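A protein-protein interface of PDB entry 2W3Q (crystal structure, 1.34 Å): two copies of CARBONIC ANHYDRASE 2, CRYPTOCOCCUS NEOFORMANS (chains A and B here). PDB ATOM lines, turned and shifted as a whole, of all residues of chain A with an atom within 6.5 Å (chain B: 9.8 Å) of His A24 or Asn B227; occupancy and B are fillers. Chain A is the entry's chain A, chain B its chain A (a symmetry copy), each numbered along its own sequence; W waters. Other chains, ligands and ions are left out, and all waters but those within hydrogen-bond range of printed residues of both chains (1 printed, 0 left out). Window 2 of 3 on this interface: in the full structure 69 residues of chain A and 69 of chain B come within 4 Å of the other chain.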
ATOM      1  N   ASP A  19      -9.896  32.960 -39.871  1.00  0.00           N
ATOM      2  CA  ASP A  19     -10.623  31.772 -40.308  1.00  0.00           C
ATOM      3  C   ASP A  19      -9.847  30.532 -39.898  1.00  0.00           C
ATOM      4  O   ASP A  19     -10.431  29.565 -39.456  1.00  0.00           O
ATOM      5  CB  ASP A  19     -10.835  31.715 -41.816  1.00  0.00           C
ATOM      6  CG  ASP A  19     -11.812  32.671 -42.410  1.00  0.00           C
ATOM      7  OD1 ASP A  19     -12.626  33.304 -41.709  1.00  0.00           O
ATOM      8  OD2 ASP A  19     -11.761  32.779 -43.649  1.00  0.00           O
ATOM      9  N   MET A  20      -8.529  30.598 -40.129  1.00  0.00           N
ATOM     10  CA  MET A  20      -7.788  29.395 -39.771  1.00  0.00           C
ATOM     11  C   MET A  20      -7.818  29.185 -38.259  1.00  0.00           C
ATOM     12  O   MET A  20      -7.982  28.079 -37.730  1.00  0.00           O
ATOM     13  CB  MET A  20      -6.369  29.470 -40.320  1.00  0.00           C
ATOM     14  CG  MET A  20      -6.331  29.183 -41.844  1.00  0.00           C
ATOM     15  SD  MET A  20      -4.632  29.560 -42.390  1.00  0.00           S
ATOM     16  N   ASP A  21      -7.656  30.262 -37.507  1.00  0.00           N
ATOM     17  CA  ASP A  21      -7.716  30.171 -36.051  1.00  0.00           C
ATOM     18  C   ASP A  21      -9.032  29.625 -35.542  1.00  0.00           C
ATOM     19  O   ASP A  21      -9.039  28.980 -34.488  1.00  0.00           O
ATOM     20  CB  ASP A  21      -7.520  31.526 -35.390  1.00  0.00           C
ATOM     21  CG  ASP A  21      -6.273  32.273 -35.770  1.00  0.00           C
ATOM     22  OD1 ASP A  21      -5.220  31.587 -35.907  1.00  0.00           O
ATOM     23  OD2 ASP A  21      -6.360  33.526 -35.908  1.00  0.00           O
ATOM     24  N   LEU A  22     -10.104  29.908 -36.249  1.00  0.00           N
ATOM     25  CA  LEU A  22     -11.389  29.388 -35.774  1.00  0.00           C
ATOM     26  C   LEU A  22     -11.710  27.991 -36.267  1.00  0.00           C
ATOM     27  O   LEU A  22     -12.750  27.420 -35.943  1.00  0.00           O
ATOM     28  CB  LEU A  22     -12.491  30.384 -36.138  1.00  0.00           C
ATOM     29  CG  LEU A  22     -12.328  31.719 -35.402  1.00  0.00           C
ATOM     30  CD1 LEU A  22     -13.519  32.619 -35.788  1.00  0.00           C
ATOM     31  CD2 LEU A  22     -12.189  31.631 -33.886  1.00  0.00           C
ATOM     32  N   GLY A  23     -10.817  27.409 -37.051  1.00  0.00           N
ATOM     33  CA  GLY A  23     -10.967  26.053 -37.532  1.00  0.00           C
ATOM     34  C   GLY A  23     -11.110  25.071 -36.388  1.00  0.00           C
ATOM     35  O   GLY A  23     -11.743  24.032 -36.535  1.00  0.00           O
ATOM     36  N   HIS A  24     -10.525  25.432 -35.249  1.00  0.00           N
ATOM     37  CA  HIS A  24     -10.648  24.520 -34.125  1.00  0.00           C
ATOM     38  C   HIS A  24     -12.098  24.381 -33.675  1.00  0.00           C
ATOM     39  O   HIS A  24     -12.509  23.361 -33.095  1.00  0.00           O
ATOM     40  CB  HIS A  24      -9.780  24.958 -32.946  1.00  0.00           C
ATOM     41  CG  HIS A  24     -10.376  26.075 -32.160  1.00  0.00           C
ATOM     42  ND1 HIS A  24     -10.247  27.382 -32.548  1.00  0.00           N
ATOM     43  CD2 HIS A  24     -11.113  26.079 -31.028  1.00  0.00           C
ATOM     44  CE1 HIS A  24     -10.893  28.125 -31.682  1.00  0.00           C
ATOM     45  NE2 HIS A  24     -11.418  27.384 -30.735  1.00  0.00           N
ATOM     46  N   SER A  25     -12.914  25.385 -33.916  1.00  0.00           N
ATOM     47  CA  SER A  25     -14.283  25.386 -33.438  1.00  0.00           C
ATOM     48  C   SER A  25     -15.287  24.701 -34.363  1.00  0.00           C
ATOM     49  O   SER A  25     -15.509  25.196 -35.453  1.00  0.00           O
ATOM     50  CB  SER A  25     -14.802  26.790 -33.166  1.00  0.00           C
ATOM     51  OG  SER A  25     -16.165  26.781 -32.813  1.00  0.00           O
ATOM     52  N   VAL A  26     -15.926  23.605 -34.030  1.00  0.00           N
ATOM     53  CA  VAL A  26     -16.910  22.796 -34.688  1.00  0.00           C
ATOM     54  C   VAL A  26     -18.105  23.722 -34.872  1.00  0.00           C
ATOM     55  O   VAL A  26     -18.564  23.895 -35.987  1.00  0.00           O
ATOM     56  CB  VAL A  26     -17.288  21.498 -33.946  1.00  0.00           C
ATOM     57  CG1 VAL A  26     -18.393  20.757 -34.691  1.00  0.00           C
ATOM     58  CG2 VAL A  26     -16.056  20.602 -33.813  1.00  0.00           C
ATOM     59  N   ALA A  27     -18.568  24.307 -33.760  1.00  0.00           N
ATOM     60  CA  ALA A  27     -19.753  25.154 -33.875  1.00  0.00           C
ATOM     61  C   ALA A  27     -19.530  26.347 -34.764  1.00  0.00           C
ATOM     62  O   ALA A  27     -20.491  26.741 -35.425  1.00  0.00           O
ATOM     63  CB  ALA A  27     -20.222  25.649 -32.535  1.00  0.00           C
ATOM     64  N   GLN A  29     -18.164  26.426 -37.488  1.00  0.00           N
ATOM     65  CA  GLN A  29     -18.338  26.013 -38.847  1.00  0.00           C
ATOM     66  C   GLN A  29     -19.804  25.802 -39.170  1.00  0.00           C
ATOM     67  O   GLN A  29     -20.153  25.800 -40.342  1.00  0.00           O
ATOM     68  CB  GLN A  29     -17.599  24.701 -39.100  1.00  0.00           C
ATOM     69  CG  GLN A  29     -16.154  24.656 -38.600  1.00  0.00           C
ATOM     70  CD  GLN A  29     -15.250  25.785 -38.998  1.00  0.00           C
ATOM     71  OE1 GLN A  29     -14.646  26.466 -38.141  1.00  0.00           O
ATOM     72  NE2 GLN A  29     -15.111  25.995 -40.295  1.00  0.00           N
ATOM     73  N   LEU A  38     -17.153  34.966 -32.485  1.00  0.00           N
ATOM     74  CA  LEU A  38     -15.744  34.577 -32.287  1.00  0.00           C
ATOM     75  C   LEU A  38     -14.831  35.429 -33.124  1.00  0.00           C
ATOM     76  O   LEU A  38     -13.732  35.785 -32.690  1.00  0.00           O
ATOM     77  CB  LEU A  38     -15.626  33.085 -32.547  1.00  0.00           C
ATOM     78  CG  LEU A  38     -16.245  32.201 -31.466  1.00  0.00           C
ATOM     79  CD1 LEU A  38     -16.148  30.765 -31.942  1.00  0.00           C
ATOM     80  CD2 LEU A  38     -15.565  32.381 -30.114  1.00  0.00           C
ATOM     81  N   ARG A  42     -11.640  37.750 -31.936  1.00  0.00           N
ATOM     82  CA  ARG A  42     -10.299  37.661 -32.515  1.00  0.00           C
ATOM     83  C   ARG A  42      -9.852  39.022 -33.046  1.00  0.00           C
ATOM     84  O   ARG A  42      -8.676  39.359 -32.857  1.00  0.00           O
ATOM     85  CB  ARG A  42     -10.229  36.609 -33.638  1.00  0.00           C
ATOM     86  CG  ARG A  42     -10.332  35.161 -33.208  1.00  0.00           C
ATOM     87  CD  ARG A  42      -9.128  34.788 -32.361  1.00  0.00           C
ATOM     88  NE  ARG A  42      -9.105  33.425 -31.853  1.00  0.00           N
ATOM     89  CZ  ARG A  42      -9.916  32.695 -31.159  1.00  0.00           C
ATOM     90  NH1 ARG A  42     -11.106  33.065 -30.739  1.00  0.00           N
ATOM     91  NH2 ARG A  42      -9.616  31.439 -30.821  1.00  0.00           N
ATOM     92  N   VAL B 125     -21.342  28.616 -21.733  1.00  0.00           N
ATOM     93  CA  VAL B 125     -20.632  28.705 -20.481  1.00  0.00           C
ATOM     94  C   VAL B 125     -19.188  29.053 -20.816  1.00  0.00           C
ATOM     95  O   VAL B 125     -18.551  28.380 -21.626  1.00  0.00           O
ATOM     96  CB  VAL B 125     -20.669  27.377 -19.723  1.00  0.00           C
ATOM     97  CG1 VAL B 125     -19.903  27.545 -18.407  1.00  0.00           C
ATOM     98  CG2 VAL B 125     -22.099  26.904 -19.511  1.00  0.00           C
ATOM     99  N   LYS B 178     -11.009  24.125 -17.420  1.00  0.00           N
ATOM    100  CA  LYS B 178     -11.695  23.564 -18.574  1.00  0.00           C
ATOM    101  C   LYS B 178     -12.757  22.537 -18.176  1.00  0.00           C
ATOM    102  O   LYS B 178     -13.887  22.516 -18.684  1.00  0.00           O
ATOM    103  CB  LYS B 178     -10.678  22.952 -19.541  1.00  0.00           C
ATOM    104  CG  LYS B 178      -9.906  24.022 -20.310  1.00  0.00           C
ATOM    105  CD  LYS B 178      -9.045  23.445 -21.424  1.00  0.00           C
ATOM    106  CE  LYS B 178      -7.620  23.972 -21.371  1.00  0.00           C
ATOM    107  NZ  LYS B 178      -6.761  23.151 -22.270  1.00  0.00           N
ATOM    108  N   VAL B 181     -15.815  24.202 -16.816  1.00  0.00           N
ATOM    109  CA  VAL B 181     -16.700  24.627 -17.924  1.00  0.00           C
ATOM    110  C   VAL B 181     -17.579  23.467 -18.374  1.00  0.00           C
ATOM    111  O   VAL B 181     -18.802  23.579 -18.536  1.00  0.00           O
ATOM    112  CB  VAL B 181     -15.925  25.210 -19.105  1.00  0.00           C
ATOM    113  CG1 VAL B 181     -16.868  25.467 -20.277  1.00  0.00           C
ATOM    114  CG2 VAL B 181     -15.222  26.499 -18.700  1.00  0.00           C
ATOM    115  N   LYS B 182     -16.962  22.310 -18.622  1.00  0.00           N
ATOM    116  CA  LYS B 182     -17.681  21.163 -19.146  1.00  0.00           C
ATOM    117  C   LYS B 182     -18.716  20.673 -18.150  1.00  0.00           C
ATOM    118  O   LYS B 182     -19.782  20.232 -18.548  1.00  0.00           O
ATOM    119  CB  LYS B 182     -16.675  20.052 -19.476  1.00  0.00           C
ATOM    120  CG  LYS B 182     -15.676  20.424 -20.564  1.00  0.00           C
ATOM    121  CD  LYS B 182     -14.677  19.371 -20.955  1.00  0.00           C
ATOM    122  CE  LYS B 182     -13.724  19.788 -22.057  1.00  0.00           C
ATOM    123  NZ  LYS B 182     -12.851  18.689 -22.588  1.00  0.00           N
ATOM    124  N   VAL B 185     -21.662  23.043 -18.407  1.00  0.00           N
ATOM    125  CA  VAL B 185     -22.395  22.761 -19.640  1.00  0.00           C
ATOM    126  C   VAL B 185     -23.316  21.584 -19.383  1.00  0.00           C
ATOM    127  O   VAL B 185     -24.501  21.574 -19.753  1.00  0.00           O
ATOM    128  CB  VAL B 185     -21.429  22.452 -20.792  1.00  0.00           C
ATOM    129  CG1 VAL B 185     -22.136  21.805 -21.968  1.00  0.00           C
ATOM    130  CG2 VAL B 185     -20.738  23.725 -21.275  1.00  0.00           C
ATOM    131  N   VAL B 211     -26.061  24.450 -26.459  1.00  0.00           N
ATOM    132  CA  VAL B 211     -25.249  24.773 -25.285  1.00  0.00           C
ATOM    133  C   VAL B 211     -23.796  24.534 -25.656  1.00  0.00           C
ATOM    134  O   VAL B 211     -23.499  23.506 -26.262  1.00  0.00           O
ATOM    135  CB  VAL B 211     -25.616  23.926 -24.056  1.00  0.00           C
ATOM    136  CG1 VAL B 211     -24.917  24.471 -22.826  1.00  0.00           C
ATOM    137  CG2 VAL B 211     -27.121  23.897 -23.803  1.00  0.00           C
ATOM    138  N   HIS B 212     -22.920  25.455 -25.335  1.00  0.00           N
ATOM    139  CA  HIS B 212     -21.509  25.436 -25.708  1.00  0.00           C
ATOM    140  C   HIS B 212     -20.630  25.678 -24.505  1.00  0.00           C
ATOM    141  O   HIS B 212     -21.063  26.325 -23.538  1.00  0.00           O
ATOM    142  CB  HIS B 212     -21.264  26.603 -26.679  1.00  0.00           C
ATOM    143  CG  HIS B 212     -22.143  26.647 -27.871  1.00  0.00           C
ATOM    144  ND1 HIS B 212     -23.347  27.301 -27.966  1.00  0.00           N
ATOM    145  CD2 HIS B 212     -21.923  26.053 -29.051  1.00  0.00           C
ATOM    146  CE1 HIS B 212     -23.798  27.080 -29.201  1.00  0.00           C
ATOM    147  NE2 HIS B 212     -22.970  26.347 -29.879  1.00  0.00           N
ATOM    148  N   GLY B 213     -19.381  25.225 -24.598  1.00  0.00           N
ATOM    149  CA  GLY B 213     -18.409  25.486 -23.590  1.00  0.00           C
ATOM    150  C   GLY B 213     -17.171  26.150 -24.154  1.00  0.00           C
ATOM    151  O   GLY B 213     -16.543  25.616 -25.048  1.00  0.00           O
ATOM    152  N   TRP B 214     -16.849  27.310 -23.615  1.00  0.00           N
ATOM    153  CA  TRP B 214     -15.766  28.142 -24.064  1.00  0.00           C
ATOM    154  C   TRP B 214     -14.792  28.469 -22.937  1.00  0.00           C
ATOM    155  O   TRP B 214     -15.160  28.417 -21.775  1.00  0.00           O
ATOM    156  CB  TRP B 214     -16.339  29.461 -24.587  1.00  0.00           C
ATOM    157  CG  TRP B 214     -17.079  29.396 -25.877  1.00  0.00           C
ATOM    158  CD1 TRP B 214     -17.317  28.335 -26.691  1.00  0.00           C
ATOM    159  CD2 TRP B 214     -17.697  30.525 -26.513  1.00  0.00           C
ATOM    160  NE1 TRP B 214     -18.043  28.742 -27.794  1.00  0.00           N
ATOM    161  CE2 TRP B 214     -18.287  30.095 -27.692  1.00  0.00           C
ATOM    162  CE3 TRP B 214     -17.804  31.881 -26.169  1.00  0.00           C
ATOM    163  CZ2 TRP B 214     -18.962  30.994 -28.518  1.00  0.00           C
ATOM    164  CZ3 TRP B 214     -18.474  32.747 -27.000  1.00  0.00           C
ATOM    165  CH2 TRP B 214     -19.062  32.304 -28.181  1.00  0.00           C
ATOM    166  N   LEU B 215     -13.573  28.837 -23.327  1.00  0.00           N
ATOM    167  CA  LEU B 215     -12.546  29.246 -22.409  1.00  0.00           C
ATOM    168  C   LEU B 215     -11.891  30.544 -22.856  1.00  0.00           C
ATOM    169  O   LEU B 215     -11.371  30.593 -23.968  1.00  0.00           O
ATOM    170  CB  LEU B 215     -11.463  28.160 -22.276  1.00  0.00           C
ATOM    171  CG  LEU B 215     -10.278  28.461 -21.371  1.00  0.00           C
ATOM    172  CD1 LEU B 215     -10.689  28.336 -19.932  1.00  0.00           C
ATOM    173  CD2 LEU B 215      -9.134  27.487 -21.675  1.00  0.00           C
ATOM    174  N   TYR B 216     -11.913  31.558 -22.018  1.00  0.00           N
ATOM    175  CA  TYR B 216     -11.234  32.809 -22.330  1.00  0.00           C
ATOM    176  C   TYR B 216      -9.808  32.766 -21.795  1.00  0.00           C
ATOM    177  O   TYR B 216      -9.575  32.625 -20.595  1.00  0.00           O
ATOM    178  CB  TYR B 216     -12.000  33.986 -21.745  1.00  0.00           C
ATOM    179  CG  TYR B 216     -11.332  35.338 -21.947  1.00  0.00           C
ATOM    180  CD1 TYR B 216     -10.997  35.809 -23.208  1.00  0.00           C
ATOM    181  CD2 TYR B 216     -11.037  36.185 -20.885  1.00  0.00           C
ATOM    182  CE1 TYR B 216     -10.406  37.035 -23.419  1.00  0.00           C
ATOM    183  CE2 TYR B 216     -10.434  37.400 -21.095  1.00  0.00           C
ATOM    184  CZ  TYR B 216     -10.109  37.841 -22.351  1.00  0.00           C
ATOM    185  OH  TYR B 216      -9.503  39.078 -22.503  1.00  0.00           O
ATOM    186  N   ASN B 222      -7.829  35.571 -26.494  1.00  0.00           N
ATOM    187  CA  ASN B 222      -8.626  34.727 -27.320  1.00  0.00           C
ATOM    188  C   ASN B 222      -9.597  33.837 -26.548  1.00  0.00           C
ATOM    189  O   ASN B 222      -9.271  33.222 -25.542  1.00  0.00           O
ATOM    190  CB  ASN B 222      -7.766  33.836 -28.199  1.00  0.00           C
ATOM    191  CG  ASN B 222      -6.949  34.643 -29.208  1.00  0.00           C
ATOM    192  OD1 ASN B 222      -7.449  35.614 -29.746  1.00  0.00           O
ATOM    193  ND2 ASN B 222      -5.721  34.197 -29.421  1.00  0.00           N
ATOM    194  N   ILE B 223     -10.817  33.600 -26.927  1.00  0.00           N
ATOM    195  CA  ILE B 223     -11.831  32.686 -26.639  1.00  0.00           C
ATOM    196  C   ILE B 223     -11.540  31.426 -27.487  1.00  0.00           C
ATOM    197  O   ILE B 223     -11.458  31.512 -28.723  1.00  0.00           O
ATOM    198  CB  ILE B 223     -13.264  33.184 -26.841  1.00  0.00           C
ATOM    199  CG1 ILE B 223     -13.651  34.140 -25.680  1.00  0.00           C
ATOM    200  CG2 ILE B 223     -14.223  32.020 -26.871  1.00  0.00           C
ATOM    201  CD1 ILE B 223     -14.554  35.253 -26.116  1.00  0.00           C
ATOM    202  N   VAL B 224     -11.401  30.331 -26.726  1.00  0.00           N
ATOM    203  CA  VAL B 224     -11.266  29.042 -27.389  1.00  0.00           C
ATOM    204  C   VAL B 224     -12.516  28.194 -27.143  1.00  0.00           C
ATOM    205  O   VAL B 224     -13.030  28.126 -26.033  1.00  0.00           O
ATOM    206  CB  VAL B 224      -9.998  28.255 -27.009  1.00  0.00           C
ATOM    207  CG1 VAL B 224      -8.768  29.158 -27.066  1.00  0.00           C
ATOM    208  CG2 VAL B 224     -10.104  27.555 -25.686  1.00  0.00           C
ATOM    209  N   ASP B 225     -13.000  27.560 -28.183  1.00  0.00           N
ATOM    210  CA  ASP B 225     -14.118  26.625 -28.094  1.00  0.00           C
ATOM    211  C   ASP B 225     -13.604  25.269 -27.597  1.00  0.00           C
ATOM    212  O   ASP B 225     -12.710  24.663 -28.193  1.00  0.00           O
ATOM    213  CB  ASP B 225     -14.783  26.481 -29.434  1.00  0.00           C
ATOM    214  CG  ASP B 225     -16.141  25.819 -29.421  1.00  0.00           C
ATOM    215  OD1 ASP B 225     -16.459  25.193 -28.385  1.00  0.00           O
ATOM    216  OD2 ASP B 225     -16.834  25.926 -30.448  1.00  0.00           O
ATOM    217  N   LEU B 226     -14.145  24.795 -26.486  1.00  0.00           N
ATOM    218  CA  LEU B 226     -13.809  23.488 -25.938  1.00  0.00           C
ATOM    219  C   LEU B 226     -14.462  22.309 -26.660  1.00  0.00           C
ATOM    220  O   LEU B 226     -14.200  21.151 -26.376  1.00  0.00           O
ATOM    221  CB  LEU B 226     -14.120  23.416 -24.438  1.00  0.00           C
ATOM    222  CG  LEU B 226     -13.446  24.500 -23.575  1.00  0.00           C
ATOM    223  CD1 LEU B 226     -13.827  24.363 -22.100  1.00  0.00           C
ATOM    224  CD2 LEU B 226     -11.935  24.462 -23.763  1.00  0.00           C
ATOM    225  N   ASN B 227     -15.328  22.603 -27.612  1.00  0.00           N
ATOM    226  CA  ASN B 227     -16.008  21.602 -28.419  1.00  0.00           C
ATOM    227  C   ASN B 227     -16.787  20.561 -27.648  1.00  0.00           C
ATOM    228  O   ASN B 227     -16.589  19.358 -27.824  1.00  0.00           O
ATOM    229  CB  ASN B 227     -14.993  20.953 -29.381  1.00  0.00           C
ATOM    230  CG  ASN B 227     -14.320  21.860 -30.346  1.00  0.00           C
ATOM    231  OD1 ASN B 227     -13.151  21.941 -30.669  1.00  0.00           O
ATOM    232  ND2 ASN B 227     -15.112  22.717 -30.921  1.00  0.00           N
ATOM    233  N   VAL B 228     -17.667  21.132 -26.833  1.00  0.00           N
ATOM    234  CA  VAL B 228     -18.597  20.308 -26.062  1.00  0.00           C
ATOM    235  C   VAL B 228     -20.024  20.708 -26.363  1.00  0.00           C
ATOM    236  O   VAL B 228     -20.924  20.565 -25.553  1.00  0.00           O
ATOM    237  CB  VAL B 228     -18.226  20.366 -24.586  1.00  0.00           C
ATOM    238  CG1 VAL B 228     -16.875  19.701 -24.362  1.00  0.00           C
ATOM    239  CG2 VAL B 228     -18.206  21.792 -24.030  1.00  0.00           C
ATOM    240  N   THR B 229     -20.253  21.221 -27.555  1.00  0.00           N
ATOM    241  CA  THR B 229     -21.589  21.700 -27.905  1.00  0.00           C
ATOM    242  C   THR B 229     -22.621  20.576 -27.996  1.00  0.00           C
ATOM    243  O   THR B 229     -22.342  19.503 -28.559  1.00  0.00           O
ATOM    244  CB  THR B 229     -21.551  22.457 -29.262  1.00  0.00           C
ATOM    245  OG1 THR B 229     -20.662  23.570 -29.135  1.00  0.00           O
ATOM    246  CG2 THR B 229     -22.937  22.944 -29.694  1.00  0.00           C
ATOM    247  N   GLN B 230     -23.815  20.823 -27.466  1.00  0.00           N
ATOM    248  CA  GLN B 230     -24.948  19.915 -27.566  1.00  0.00           C
ATOM    249  C   GLN B 230     -26.195  20.700 -27.997  1.00  0.00           C
ATOM    250  O   GLN B 230     -26.361  21.873 -27.642  1.00  0.00           O
ATOM    251  CB  GLN B 230     -25.238  19.218 -26.259  1.00  0.00           C
ATOM    252  CG  GLN B 230     -24.100  18.346 -25.738  1.00  0.00           C
ATOM    253  CD  GLN B 230     -24.577  17.499 -24.560  1.00  0.00           C
ATOM    254  OE1 GLN B 230     -25.606  16.803 -24.604  1.00  0.00           O
ATOM    255  NE2 GLN B 230     -23.822  17.566 -23.485  1.00  0.00           N
HETATM  256  O   HOH W   1     -17.984  23.502 -31.000  1.00  0.00           O
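No position is printed for both chains. Of the 12 pairs that touch across the chains among the printed residues, none has its exchanged pair printed and touching as well.
Of the 12 printed residues of chain A, 6 touch a printed residue of chain B. Among the printed residues, no Asp or Glu carboxylate lies within 4 Å of a Lys or Arg side-chain nitrogen of the other chain.
N of Asp B225 sits at hydrogen-bond distance from NE2 of His A24 (3.0 Å). The guanidinium group of Arg A42 sits close to the side-chain amide oxygen of Asn B222 (3.5 Å). The backbone carbonyl oxygen (O) of His A24 lies close to the side-chain amide oxygen (OD1) of Asn B227 (2.9 Å). The side-chain carboxylate (OD2) of Asp B225 lies within hydrogen-bond range of the side-chain hydroxyl (OG) of Ser A25 (2.6 Å). The side-chain amide nitrogen (ND2) of Asn B227 sits close to the backbone NH (N) of Val A26, 3.3 Å away. The guanidinium group (NH1) of Arg A42 lies within hydrogen-bond range of the backbone carbonyl oxygen (O) of Ile B223.
The backbone carbonyl oxygen (O) of Leu B215 is in hydrogen-bond range of the backbone NH (N) of Val B224, 2.8 Å away. N of Asn B227 is in hydrogen-bond range of OD1 of Asp B225, 2.9 Å away. The backbone carbonyl oxygen (O) of Val B125 is in hydrogen-bond range of the backbone NH (N) of Trp B214, 2.8 Å away. OE1 of Gln A29 lies close to O of Ser A25 (3.1 Å). N of Val B125 is in hydrogen-bond range of O of His B212. A ring nitrogen (ND1) of His A24 lies within hydrogen-bond range of the backbone carbonyl oxygen (O) of Asp A21 (2.8 Å).
Among the printed residues, merely in contact across the chains: Leu A38 with Ile B223, His A24 with Val B224, Ser A25 with Asn B227, Ala A27 with His B212, Ala A27 with Asp B225 and Leu A38 with Trp B214.
Of chain B, only Val B224, Asp B225 and Asn B227 come within 4 Å of His A24. Of the printed residues of chain B, Ser A25 touches Asp B225 (2.6 Å) and Asn B227 (3.8 Å). Printed residues of chain B within 4 Å of Ala A27: His B212 and Asp B225. Printed residues of chain B within 4 Å of Arg A42: Asn B222 and Ile B223. Of the printed residues of chain A, Trp B214 touches Leu A38. Of the printed residues of chain A, Asn B222 touches Arg A42. Printed residues of chain A within 4 Å of Ile B223: Leu A38 (3.5 Å) and Arg A42 (2.6 Å). Leu B226 touches none of the printed residues of chain A. Of chain A, only His A24, Ser A25 and Val A26 come within 4 Å of Asn B227. Thr B229 touches none of the printed residues of chain A. The nearest printed residue of chain B that does not touch Val A26 is Asp B225 (4.4 Å).
Water W1 lies within hydrogen-bond range of the side-chain carboxylate of Asp B225 (2.7 Å), the backbone NH of Ala A27 (2.9 Å), the side-chain amide nitrogen of Asn B227 (3.0 Å) and the side-chain hydroxyl of Thr B229 (3.3 Å).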
